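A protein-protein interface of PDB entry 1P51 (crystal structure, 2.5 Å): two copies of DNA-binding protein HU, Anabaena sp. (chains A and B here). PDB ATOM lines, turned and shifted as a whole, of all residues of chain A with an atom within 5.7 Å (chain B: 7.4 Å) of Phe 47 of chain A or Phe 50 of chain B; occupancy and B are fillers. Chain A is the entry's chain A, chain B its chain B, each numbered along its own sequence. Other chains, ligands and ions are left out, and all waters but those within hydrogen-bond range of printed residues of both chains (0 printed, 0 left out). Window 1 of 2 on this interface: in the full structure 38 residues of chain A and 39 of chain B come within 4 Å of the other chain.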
ATOM      1  N   LEU A  44      14.120   7.579 -10.755  1.00  0.00           N
ATOM      2  CA  LEU A  44      15.556   7.797 -10.872  1.00  0.00           C
ATOM      3  C   LEU A  44      16.291   6.768 -10.025  1.00  0.00           C
ATOM      4  O   LEU A  44      16.268   6.832  -8.793  1.00  0.00           O
ATOM      5  CB  LEU A  44      15.934   9.222 -10.441  1.00  0.00           C
ATOM      6  CG  LEU A  44      15.155  10.405 -11.029  1.00  0.00           C
ATOM      7  CD1 LEU A  44      15.555  11.701 -10.340  1.00  0.00           C
ATOM      8  CD2 LEU A  44      15.364  10.509 -12.536  1.00  0.00           C
ATOM      9  N   VAL A  45      16.931   5.814 -10.698  1.00  0.00           N
ATOM     10  CA  VAL A  45      17.651   4.732 -10.029  1.00  0.00           C
ATOM     11  C   VAL A  45      18.654   5.269  -9.012  1.00  0.00           C
ATOM     12  O   VAL A  45      19.280   6.310  -9.232  1.00  0.00           O
ATOM     13  CB  VAL A  45      18.359   3.785 -11.038  1.00  0.00           C
ATOM     14  CG1 VAL A  45      17.341   2.913 -11.758  1.00  0.00           C
ATOM     15  CG2 VAL A  45      19.208   4.568 -12.039  1.00  0.00           C
ATOM     16  N   GLY A  46      18.782   4.561  -7.893  1.00  0.00           N
ATOM     17  CA  GLY A  46      19.666   4.974  -6.818  1.00  0.00           C
ATOM     18  C   GLY A  46      19.025   6.023  -5.935  1.00  0.00           C
ATOM     19  O   GLY A  46      18.908   5.835  -4.722  1.00  0.00           O
ATOM     20  N   PHE A  47      18.603   7.126  -6.553  1.00  0.00           N
ATOM     21  CA  PHE A  47      17.987   8.244  -5.843  1.00  0.00           C
ATOM     22  C   PHE A  47      16.599   7.889  -5.321  1.00  0.00           C
ATOM     23  O   PHE A  47      16.426   7.652  -4.125  1.00  0.00           O
ATOM     24  CB  PHE A  47      17.923   9.483  -6.746  1.00  0.00           C
ATOM     25  CG  PHE A  47      17.557  10.748  -6.019  1.00  0.00           C
ATOM     26  CD1 PHE A  47      18.458  11.352  -5.148  1.00  0.00           C
ATOM     27  CD2 PHE A  47      16.312  11.336  -6.207  1.00  0.00           C
ATOM     28  CE1 PHE A  47      18.125  12.520  -4.474  1.00  0.00           C
ATOM     29  CE2 PHE A  47      15.970  12.509  -5.538  1.00  0.00           C
ATOM     30  CZ  PHE A  47      16.879  13.102  -4.670  1.00  0.00           C
ATOM     31  N   GLY A  48      15.620   7.849  -6.220  1.00  0.00           N
ATOM     32  CA  GLY A  48      14.246   7.571  -5.849  1.00  0.00           C
ATOM     33  C   GLY A  48      13.245   7.870  -6.946  1.00  0.00           C
ATOM     34  O   GLY A  48      13.614   8.055  -8.108  1.00  0.00           O
ATOM     35  N   SER A  49      11.968   7.916  -6.571  1.00  0.00           N
ATOM     36  CA  SER A  49      10.886   8.104  -7.530  1.00  0.00           C
ATOM     37  C   SER A  49       9.817   9.065  -7.029  1.00  0.00           C
ATOM     38  O   SER A  49       9.444   9.037  -5.855  1.00  0.00           O
ATOM     39  CB  SER A  49      10.253   6.757  -7.897  1.00  0.00           C
ATOM     40  OG  SER A  49       9.704   6.119  -6.758  1.00  0.00           O
ATOM     41  N   PHE A  50       9.333   9.912  -7.932  1.00  0.00           N
ATOM     42  CA  PHE A  50       8.256  10.850  -7.625  1.00  0.00           C
ATOM     43  C   PHE A  50       6.979  10.411  -8.325  1.00  0.00           C
ATOM     44  O   PHE A  50       7.017   9.894  -9.444  1.00  0.00           O
ATOM     45  CB  PHE A  50       8.612  12.279  -8.059  1.00  0.00           C
ATOM     46  CG  PHE A  50       9.961  12.751  -7.581  1.00  0.00           C
ATOM     47  CD1 PHE A  50      11.100  12.537  -8.353  1.00  0.00           C
ATOM     48  CD2 PHE A  50      10.089  13.420  -6.369  1.00  0.00           C
ATOM     49  CE1 PHE A  50      12.349  12.971  -7.917  1.00  0.00           C
ATOM     50  CE2 PHE A  50      11.333  13.864  -5.926  1.00  0.00           C
ATOM     51  CZ  PHE A  50      12.466  13.636  -6.701  1.00  0.00           C
ATOM     52  N   PHE A  79       7.199  10.868  -2.684  1.00  0.00           N
ATOM     53  CA  PHE A  79       8.561  10.455  -2.990  1.00  0.00           C
ATOM     54  C   PHE A  79       8.875   9.112  -2.343  1.00  0.00           C
ATOM     55  O   PHE A  79       8.542   8.874  -1.181  1.00  0.00           O
ATOM     56  CB  PHE A  79       9.553  11.528  -2.520  1.00  0.00           C
ATOM     57  CG  PHE A  79      11.002  11.159  -2.713  1.00  0.00           C
ATOM     58  CD1 PHE A  79      11.567  11.135  -3.986  1.00  0.00           C
ATOM     59  CD2 PHE A  79      11.803  10.846  -1.619  1.00  0.00           C
ATOM     60  CE1 PHE A  79      12.903  10.802  -4.169  1.00  0.00           C
ATOM     61  CE2 PHE A  79      13.146  10.510  -1.791  1.00  0.00           C
ATOM     62  CZ  PHE A  79      13.695  10.489  -3.071  1.00  0.00           C
ATOM     63  N   SER A  80       9.500   8.230  -3.116  1.00  0.00           N
ATOM     64  CA  SER A  80      10.009   6.969  -2.599  1.00  0.00           C
ATOM     65  C   SER A  80      11.526   6.994  -2.690  1.00  0.00           C
ATOM     66  O   SER A  80      12.081   7.236  -3.762  1.00  0.00           O
ATOM     67  CB  SER A  80       9.452   5.794  -3.401  1.00  0.00           C
ATOM     68  OG  SER A  80       8.141   5.472  -2.985  1.00  0.00           O
ATOM     69  N   ALA A  81      12.193   6.768  -1.563  1.00  0.00           N
ATOM     70  CA  ALA A  81      13.650   6.757  -1.529  1.00  0.00           C
ATOM     71  C   ALA A  81      14.172   5.440  -2.086  1.00  0.00           C
ATOM     72  O   ALA A  81      13.720   4.367  -1.686  1.00  0.00           O
ATOM     73  CB  ALA A  81      14.156   6.980  -0.115  1.00  0.00           C
ATOM     74  N   GLY A  82      15.107   5.535  -3.027  1.00  0.00           N
ATOM     75  CA  GLY A  82      15.731   4.368  -3.615  1.00  0.00           C
ATOM     76  C   GLY A  82      16.774   3.779  -2.688  1.00  0.00           C
ATOM     77  O   GLY A  82      17.132   4.391  -1.673  1.00  0.00           O
ATOM     78  N   LYS A  83      17.268   2.597  -3.048  1.00  0.00           N
ATOM     79  CA  LYS A  83      18.191   1.839  -2.209  1.00  0.00           C
ATOM     80  C   LYS A  83      19.456   2.616  -1.849  1.00  0.00           C
ATOM     81  O   LYS A  83      19.868   2.623  -0.688  1.00  0.00           O
ATOM     82  CB  LYS A  83      18.555   0.510  -2.875  1.00  0.00           C
ATOM     83  CG  LYS A  83      19.171  -0.510  -1.931  1.00  0.00           C
ATOM     84  CD  LYS A  83      20.272  -1.293  -2.629  1.00  0.00           C
ATOM     85  CE  LYS A  83      20.478  -2.671  -2.009  1.00  0.00           C
ATOM     86  NZ  LYS A  83      19.226  -3.488  -1.968  1.00  0.00           N
ATOM     87  N   LEU A  84      20.056   3.271  -2.844  1.00  0.00           N
ATOM     88  CA  LEU A  84      21.303   4.012  -2.652  1.00  0.00           C
ATOM     89  C   LEU A  84      21.133   5.218  -1.729  1.00  0.00           C
ATOM     90  O   LEU A  84      22.038   5.556  -0.971  1.00  0.00           O
ATOM     91  CB  LEU A  84      21.901   4.439  -4.003  1.00  0.00           C
ATOM     92  CG  LEU A  84      23.284   5.109  -4.037  1.00  0.00           C
ATOM     93  CD1 LEU A  84      24.371   4.238  -3.398  1.00  0.00           C
ATOM     94  CD2 LEU A  84      23.663   5.476  -5.463  1.00  0.00           C
ATOM     95  N   PHE A  85      19.971   5.859  -1.794  1.00  0.00           N
ATOM     96  CA  PHE A  85      19.651   6.951  -0.882  1.00  0.00           C
ATOM     97  C   PHE A  85      19.532   6.415   0.549  1.00  0.00           C
ATOM     98  O   PHE A  85      20.200   6.912   1.460  1.00  0.00           O
ATOM     99  CB  PHE A  85      18.354   7.651  -1.313  1.00  0.00           C
ATOM    100  CG  PHE A  85      18.249   9.094  -0.873  1.00  0.00           C
ATOM    101  CD1 PHE A  85      19.041   9.599   0.156  1.00  0.00           C
ATOM    102  CD2 PHE A  85      17.340   9.950  -1.493  1.00  0.00           C
ATOM    103  CE1 PHE A  85      18.934  10.931   0.556  1.00  0.00           C
ATOM    104  CE2 PHE A  85      17.223  11.287  -1.100  1.00  0.00           C
ATOM    105  CZ  PHE A  85      18.022  11.776  -0.073  1.00  0.00           C
ATOM    106  N   LYS B   3      15.393   8.197 -15.785  1.00  0.00           N
ATOM    107  CA  LYS B   3      16.535   9.115 -15.816  1.00  0.00           C
ATOM    108  C   LYS B   3      16.920   9.537 -17.232  1.00  0.00           C
ATOM    109  O   LYS B   3      17.101  10.727 -17.498  1.00  0.00           O
ATOM    110  CB  LYS B   3      17.742   8.505 -15.093  1.00  0.00           C
ATOM    111  CG  LYS B   3      18.910   9.473 -14.898  1.00  0.00           C
ATOM    112  CD  LYS B   3      19.755   9.110 -13.682  1.00  0.00           C
ATOM    113  CE  LYS B   3      21.085   9.853 -13.694  1.00  0.00           C
ATOM    114  NZ  LYS B   3      22.251   8.923 -13.588  1.00  0.00           N
ATOM    115  N   LEU B  25      23.094  16.113 -13.617  1.00  0.00           N
ATOM    116  CA  LEU B  25      21.999  15.477 -12.883  1.00  0.00           C
ATOM    117  C   LEU B  25      22.516  14.410 -11.917  1.00  0.00           C
ATOM    118  O   LEU B  25      22.053  14.327 -10.779  1.00  0.00           O
ATOM    119  CB  LEU B  25      20.961  14.887 -13.849  1.00  0.00           C
ATOM    120  CG  LEU B  25      19.671  14.262 -13.297  1.00  0.00           C
ATOM    121  CD1 LEU B  25      18.782  15.290 -12.601  1.00  0.00           C
ATOM    122  CD2 LEU B  25      18.905  13.558 -14.411  1.00  0.00           C
ATOM    123  N   ALA B  28      24.073  16.300  -9.094  1.00  0.00           N
ATOM    124  CA  ALA B  28      22.996  16.899  -8.304  1.00  0.00           C
ATOM    125  C   ALA B  28      22.330  15.899  -7.357  1.00  0.00           C
ATOM    126  O   ALA B  28      22.099  16.206  -6.187  1.00  0.00           O
ATOM    127  CB  ALA B  28      21.957  17.546  -9.224  1.00  0.00           C
ATOM    128  N   LEU B  29      22.043  14.705  -7.872  1.00  0.00           N
ATOM    129  CA  LEU B  29      21.383  13.653  -7.100  1.00  0.00           C
ATOM    130  C   LEU B  29      22.305  13.038  -6.049  1.00  0.00           C
ATOM    131  O   LEU B  29      21.863  12.727  -4.943  1.00  0.00           O
ATOM    132  CB  LEU B  29      20.826  12.563  -8.026  1.00  0.00           C
ATOM    133  CG  LEU B  29      19.745  12.958  -9.044  1.00  0.00           C
ATOM    134  CD1 LEU B  29      19.497  11.816 -10.020  1.00  0.00           C
ATOM    135  CD2 LEU B  29      18.440  13.396  -8.373  1.00  0.00           C
ATOM    136  N   GLU B  30      23.580  12.870  -6.396  1.00  0.00           N
ATOM    137  CA  GLU B  30      24.576  12.329  -5.472  1.00  0.00           C
ATOM    138  C   GLU B  30      24.856  13.285  -4.310  1.00  0.00           C
ATOM    139  O   GLU B  30      25.026  12.846  -3.171  1.00  0.00           O
ATOM    140  CB  GLU B  30      25.877  11.990  -6.210  1.00  0.00           C
ATOM    141  CG  GLU B  30      25.819  10.694  -7.013  1.00  0.00           C
ATOM    142  CD  GLU B  30      26.957  10.556  -8.015  1.00  0.00           C
ATOM    143  OE1 GLU B  30      27.642  11.564  -8.310  1.00  0.00           O
ATOM    144  OE2 GLU B  30      27.167   9.430  -8.515  1.00  0.00           O
ATOM    145  N   THR B  31      24.890  14.584  -4.610  1.00  0.00           N
ATOM    146  CA  THR B  31      25.143  15.626  -3.611  1.00  0.00           C
ATOM    147  C   THR B  31      23.990  15.750  -2.611  1.00  0.00           C
ATOM    148  O   THR B  31      24.215  15.949  -1.414  1.00  0.00           O
ATOM    149  CB  THR B  31      25.409  16.978  -4.306  1.00  0.00           C
ATOM    150  OG1 THR B  31      26.492  16.831  -5.232  1.00  0.00           O
ATOM    151  CG2 THR B  31      25.934  18.015  -3.314  1.00  0.00           C
ATOM    152  N   ILE B  32      22.761  15.626  -3.109  1.00  0.00           N
ATOM    153  CA  ILE B  32      21.577  15.631  -2.252  1.00  0.00           C
ATOM    154  C   ILE B  32      21.624  14.448  -1.278  1.00  0.00           C
ATOM    155  O   ILE B  32      21.296  14.599  -0.101  1.00  0.00           O
ATOM    156  CB  ILE B  32      20.276  15.645  -3.102  1.00  0.00           C
ATOM    157  CG1 ILE B  32      20.035  17.046  -3.679  1.00  0.00           C
ATOM    158  CG2 ILE B  32      19.067  15.192  -2.272  1.00  0.00           C
ATOM    159  CD1 ILE B  32      19.112  17.088  -4.896  1.00  0.00           C
ATOM    160  N   ILE B  33      22.064  13.289  -1.768  1.00  0.00           N
ATOM    161  CA  ILE B  33      22.231  12.098  -0.932  1.00  0.00           C
ATOM    162  C   ILE B  33      23.332  12.283   0.128  1.00  0.00           C
ATOM    163  O   ILE B  33      23.118  11.970   1.304  1.00  0.00           O
ATOM    164  CB  ILE B  33      22.487  10.838  -1.807  1.00  0.00           C
ATOM    165  CG1 ILE B  33      21.235  10.463  -2.603  1.00  0.00           C
ATOM    166  CG2 ILE B  33      22.906   9.664  -0.954  1.00  0.00           C
ATOM    167  CD1 ILE B  33      21.516   9.683  -3.881  1.00  0.00           C
ATOM    168  N   ALA B  35      24.565  15.145   1.345  1.00  0.00           N
ATOM    169  CA  ALA B  35      24.166  16.198   2.278  1.00  0.00           C
ATOM    170  C   ALA B  35      23.166  15.713   3.327  1.00  0.00           C
ATOM    171  O   ALA B  35      23.372  15.922   4.522  1.00  0.00           O
ATOM    172  CB  ALA B  35      23.624  17.407   1.524  1.00  0.00           C
ATOM    173  N   VAL B  36      22.096  15.056   2.876  1.00  0.00           N
ATOM    174  CA  VAL B  36      21.100  14.460   3.771  1.00  0.00           C
ATOM    175  C   VAL B  36      21.747  13.457   4.735  1.00  0.00           C
ATOM    176  O   VAL B  36      21.466  13.476   5.937  1.00  0.00           O
ATOM    177  CB  VAL B  36      19.944  13.779   2.980  1.00  0.00           C
ATOM    178  CG1 VAL B  36      18.947  13.118   3.926  1.00  0.00           C
ATOM    179  CG2 VAL B  36      19.228  14.789   2.096  1.00  0.00           C
ATOM    180  N   ASP B  40      22.343  17.082   6.993  1.00  0.00           N
ATOM    181  CA  ASP B  40      22.018  18.414   6.490  1.00  0.00           C
ATOM    182  C   ASP B  40      20.723  18.375   5.685  1.00  0.00           C
ATOM    183  O   ASP B  40      20.542  17.508   4.828  1.00  0.00           O
ATOM    184  CB  ASP B  40      23.165  18.965   5.634  1.00  0.00           C
ATOM    185  CG  ASP B  40      23.048  20.463   5.378  1.00  0.00           C
ATOM    186  OD1 ASP B  40      23.820  20.979   4.537  1.00  0.00           O
ATOM    187  OD2 ASP B  40      22.228  21.208   5.964  1.00  0.00           O
ATOM    188  N   LYS B  41      19.820  19.308   5.978  1.00  0.00           N
ATOM    189  CA  LYS B  41      18.563  19.430   5.242  1.00  0.00           C
ATOM    190  C   LYS B  41      18.781  20.183   3.931  1.00  0.00           C
ATOM    191  O   LYS B  41      19.357  21.271   3.922  1.00  0.00           O
ATOM    192  CB  LYS B  41      17.506  20.129   6.096  1.00  0.00           C
ATOM    193  CG  LYS B  41      16.109  20.142   5.487  1.00  0.00           C
ATOM    194  CD  LYS B  41      15.137  20.933   6.347  1.00  0.00           C
ATOM    195  CE  LYS B  41      13.800  21.096   5.656  1.00  0.00           C
ATOM    196  NZ  LYS B  41      12.653  20.838   6.580  1.00  0.00           N
ATOM    197  N   VAL B  42      18.323  19.590   2.830  1.00  0.00           N
ATOM    198  CA  VAL B  42      18.459  20.190   1.505  1.00  0.00           C
ATOM    199  C   VAL B  42      17.152  20.868   1.095  1.00  0.00           C
ATOM    200  O   VAL B  42      16.141  20.203   0.878  1.00  0.00           O
ATOM    201  CB  VAL B  42      18.890  19.145   0.440  1.00  0.00           C
ATOM    202  CG1 VAL B  42      18.904  19.757  -0.960  1.00  0.00           C
ATOM    203  CG2 VAL B  42      20.258  18.569   0.772  1.00  0.00           C
ATOM    204  N   THR B  43      17.188  22.195   0.995  1.00  0.00           N
ATOM    205  CA  THR B  43      16.012  22.983   0.631  1.00  0.00           C
ATOM    206  C   THR B  43      16.111  23.540  -0.788  1.00  0.00           C
ATOM    207  O   THR B  43      17.097  24.181  -1.146  1.00  0.00           O
ATOM    208  CB  THR B  43      15.801  24.135   1.638  1.00  0.00           C
ATOM    209  OG1 THR B  43      15.649  23.595   2.958  1.00  0.00           O
ATOM    210  CG2 THR B  43      14.468  24.844   1.380  1.00  0.00           C
ATOM    211  N   LEU B  44      15.079  23.286  -1.586  1.00  0.00           N
ATOM    212  CA  LEU B  44      14.978  23.847  -2.927  1.00  0.00           C
ATOM    213  C   LEU B  44      13.620  24.515  -3.091  1.00  0.00           C
ATOM    214  O   LEU B  44      12.596  23.837  -3.221  1.00  0.00           O
ATOM    215  CB  LEU B  44      15.196  22.767  -4.000  1.00  0.00           C
ATOM    216  CG  LEU B  44      16.444  21.874  -3.887  1.00  0.00           C
ATOM    217  CD1 LEU B  44      16.383  20.706  -4.863  1.00  0.00           C
ATOM    218  CD2 LEU B  44      17.719  22.681  -4.096  1.00  0.00           C
ATOM    219  N   PHE B  47      10.270  23.625  -5.388  1.00  0.00           N
ATOM    220  CA  PHE B  47      10.283  22.169  -5.491  1.00  0.00           C
ATOM    221  C   PHE B  47      10.020  21.504  -4.141  1.00  0.00           C
ATOM    222  O   PHE B  47       8.940  20.948  -3.918  1.00  0.00           O
ATOM    223  CB  PHE B  47      11.610  21.692  -6.090  1.00  0.00           C
ATOM    224  CG  PHE B  47      11.635  20.230  -6.438  1.00  0.00           C
ATOM    225  CD1 PHE B  47      11.043  19.772  -7.609  1.00  0.00           C
ATOM    226  CD2 PHE B  47      12.267  19.314  -5.601  1.00  0.00           C
ATOM    227  CE1 PHE B  47      11.071  18.424  -7.938  1.00  0.00           C
ATOM    228  CE2 PHE B  47      12.300  17.962  -5.922  1.00  0.00           C
ATOM    229  CZ  PHE B  47      11.700  17.516  -7.093  1.00  0.00           C
ATOM    230  N   GLY B  48      11.001  21.565  -3.244  1.00  0.00           N
ATOM    231  CA  GLY B  48      10.849  20.988  -1.922  1.00  0.00           C
ATOM    232  C   GLY B  48      12.138  20.787  -1.152  1.00  0.00           C
ATOM    233  O   GLY B  48      13.201  21.269  -1.550  1.00  0.00           O
ATOM    234  N   SER B  49      12.034  20.061  -0.041  1.00  0.00           N
ATOM    235  CA  SER B  49      13.168  19.839   0.847  1.00  0.00           C
ATOM    236  C   SER B  49      13.391  18.364   1.149  1.00  0.00           C
ATOM    237  O   SER B  49      12.440  17.579   1.199  1.00  0.00           O
ATOM    238  CB  SER B  49      12.991  20.619   2.149  1.00  0.00           C
ATOM    239  OG  SER B  49      11.922  20.095   2.919  1.00  0.00           O
ATOM    240  N   PHE B  50      14.657  18.003   1.341  1.00  0.00           N
ATOM    241  CA  PHE B  50      15.044  16.653   1.730  1.00  0.00           C
ATOM    242  C   PHE B  50      15.754  16.702   3.075  1.00  0.00           C
ATOM    243  O   PHE B  50      16.560  17.600   3.327  1.00  0.00           O
ATOM    244  CB  PHE B  50      15.974  16.017   0.689  1.00  0.00           C
ATOM    245  CG  PHE B  50      15.433  16.033  -0.715  1.00  0.00           C
ATOM    246  CD1 PHE B  50      15.718  17.095  -1.572  1.00  0.00           C
ATOM    247  CD2 PHE B  50      14.663  14.976  -1.191  1.00  0.00           C
ATOM    248  CE1 PHE B  50      15.226  17.112  -2.878  1.00  0.00           C
ATOM    249  CE2 PHE B  50      14.172  14.983  -2.497  1.00  0.00           C
ATOM    250  CZ  PHE B  50      14.452  16.057  -3.339  1.00  0.00           C
ATOM    251  N   GLU B  51      15.449  15.733   3.931  1.00  0.00           N
ATOM    252  CA  GLU B  51      16.099  15.601   5.230  1.00  0.00           C
ATOM    253  C   GLU B  51      16.061  14.149   5.695  1.00  0.00           C
ATOM    254  O   GLU B  51      15.353  13.323   5.114  1.00  0.00           O
ATOM    255  CB  GLU B  51      15.442  16.524   6.268  1.00  0.00           C
ATOM    256  CG  GLU B  51      14.158  15.984   6.886  1.00  0.00           C
ATOM    257  CD  GLU B  51      13.445  16.999   7.759  1.00  0.00           C
ATOM    258  OE1 GLU B  51      14.123  17.770   8.474  1.00  0.00           O
ATOM    259  OE2 GLU B  51      12.196  17.019   7.734  1.00  0.00           O
ATOM    260  N   SER B  52      16.835  13.844   6.732  1.00  0.00           N
ATOM    261  CA  SER B  52      16.811  12.526   7.351  1.00  0.00           C
ATOM    262  C   SER B  52      15.828  12.522   8.516  1.00  0.00           C
ATOM    263  O   SER B  52      15.934  13.342   9.429  1.00  0.00           O
ATOM    264  CB  SER B  52      18.209  12.131   7.832  1.00  0.00           C
ATOM    265  OG  SER B  52      18.690  13.056   8.791  1.00  0.00           O
ATOM    266  N   PRO B  77      15.564   8.614   4.544  1.00  0.00           N
ATOM    267  CA  PRO B  77      15.393   9.841   3.758  1.00  0.00           C
ATOM    268  C   PRO B  77      13.933  10.281   3.750  1.00  0.00           C
ATOM    269  O   PRO B  77      13.026   9.443   3.768  1.00  0.00           O
ATOM    270  CB  PRO B  77      15.826   9.424   2.348  1.00  0.00           C
ATOM    271  CG  PRO B  77      16.599   8.170   2.542  1.00  0.00           C
ATOM    272  CD  PRO B  77      15.950   7.475   3.694  1.00  0.00           C
ATOM    273  N   ALA B  78      13.723  11.593   3.728  1.00  0.00           N
ATOM    274  CA  ALA B  78      12.386  12.171   3.714  1.00  0.00           C
ATOM    275  C   ALA B  78      12.308  13.268   2.664  1.00  0.00           C
ATOM    276  O   ALA B  78      13.336  13.761   2.203  1.00  0.00           O
ATOM    277  CB  ALA B  78      12.049  12.723   5.078  1.00  0.00           C
ATOM    278  N   PHE B  79      11.083  13.638   2.292  1.00  0.00           N
ATOM    279  CA  PHE B  79      10.835  14.705   1.325  1.00  0.00           C
ATOM    280  C   PHE B  79       9.609  15.526   1.714  1.00  0.00           C
ATOM    281  O   PHE B  79       8.570  14.973   2.094  1.00  0.00           O
ATOM    282  CB  PHE B  79      10.654  14.132  -0.088  1.00  0.00           C
ATOM    283  CG  PHE B  79      10.308  15.169  -1.132  1.00  0.00           C
ATOM    284  CD1 PHE B  79      11.264  16.091  -1.565  1.00  0.00           C
ATOM    285  CD2 PHE B  79       9.032  15.226  -1.680  1.00  0.00           C
ATOM    286  CE1 PHE B  79      10.950  17.052  -2.530  1.00  0.00           C
ATOM    287  CE2 PHE B  79       8.710  16.182  -2.645  1.00  0.00           C
ATOM    288  CZ  PHE B  79       9.673  17.095  -3.069  1.00  0.00           C
ATOM    289  N   SER B  80       9.745  16.847   1.622  1.00  0.00           N
ATOM    290  CA  SER B  80       8.620  17.756   1.806  1.00  0.00           C
ATOM    291  C   SER B  80       8.410  18.552   0.530  1.00  0.00           C
ATOM    292  O   SER B  80       9.340  19.178   0.021  1.00  0.00           O
ATOM    293  CB  SER B  80       8.862  18.698   2.986  1.00  0.00           C
ATOM    294  OG  SER B  80       8.343  18.147   4.190  1.00  0.00           O
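O of Gly 46 of chain A lies within hydrogen-bond range of N of Phe 85 of chain A (3.1 Å).
O of Phe 47 of chain A sits at hydrogen-bond distance from N of Gly 82 of chain A (2.7 Å).
The backbone carbonyl oxygen (O) of Val 42 of chain B is in hydrogen-bond range of the backbone NH (N) of Phe 50 of chain B (2.7 Å).
Among the printed residues, pairs that only touch across the chains: Phe 47 of chain A with Ile 32 of chain B (3.6 Å), Phe 85 of chain A with Ile 33 of chain B (3.6 Å), Phe 47 of chain A with Leu 29 of chain B (3.7 Å), Phe 85 of chain A with Pro 77 of chain B (3.7 Å), Phe 47 of chain A with Ile 33 of chain B (3.7 Å), Phe 79 of chain A with Phe 79 of chain B (3.7 Å), Leu 44 of chain A with Lys 3 of chain B (3.8 Å), Ala 81 of chain A with Pro 77 of chain B (3.8 Å), Phe 50 of chain A with Phe 47 of chain B (3.9 Å), Phe 85 of chain A with Val 36 of chain B (3.9 Å), Leu 44 of chain A with Leu 29 of chain B (3.9 Å) and Phe 47 of chain A with Phe 50 of chain B (3.9 Å).
No residue of chain B comes within 4 Å of Gly 46 of chain A.
Of the printed residues of chain B, Phe 50 of chain A touches Phe 47 (3.9 Å).
Thr 43 of chain B touches none of the printed residues of chain A.
Leu 44 of chain B touches none of the printed residues of chain A.
Of chain A, only Phe 47 comes within 4 Å of Phe 50 of chain B.
Printed residues of chain A within 4 Å of Pro 77 of chain B: Ala 81 (3.8 Å) and Phe 85 (3.7 Å).
The nearest residue of chain A that does not touch Phe 50 of chain B is Phe 85 of chain A (4.5 Å).
Of the 14 printed residues of chain A, 6 touch a printed residue of chain B.
Hydrophobic or aromatic side chains of chain A that line the printed part of chain B: Leu 44, Phe 47, Phe 50, Phe 79, Ala 81 and Phe 85.
Among the printed residues, no Asp or Glu carboxylate lies within 4 Å of a Lys or Arg side-chain nitrogen of the other chain.
Phe 47 of chain A touches Phe 50 of chain B, and with the chains exchanged Phe 50 of chain A touches Phe 47 of chain B.
Phe 79 of chain B touches its own counterpart, Phe 79 of chain A.
Positions printed for both chains: 44, 47, 48, 49, 50, 79 and 80.
Of the 12 pairs that touch across the chains among the printed residues, 3 have their exchanged pair printed and touching as well.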
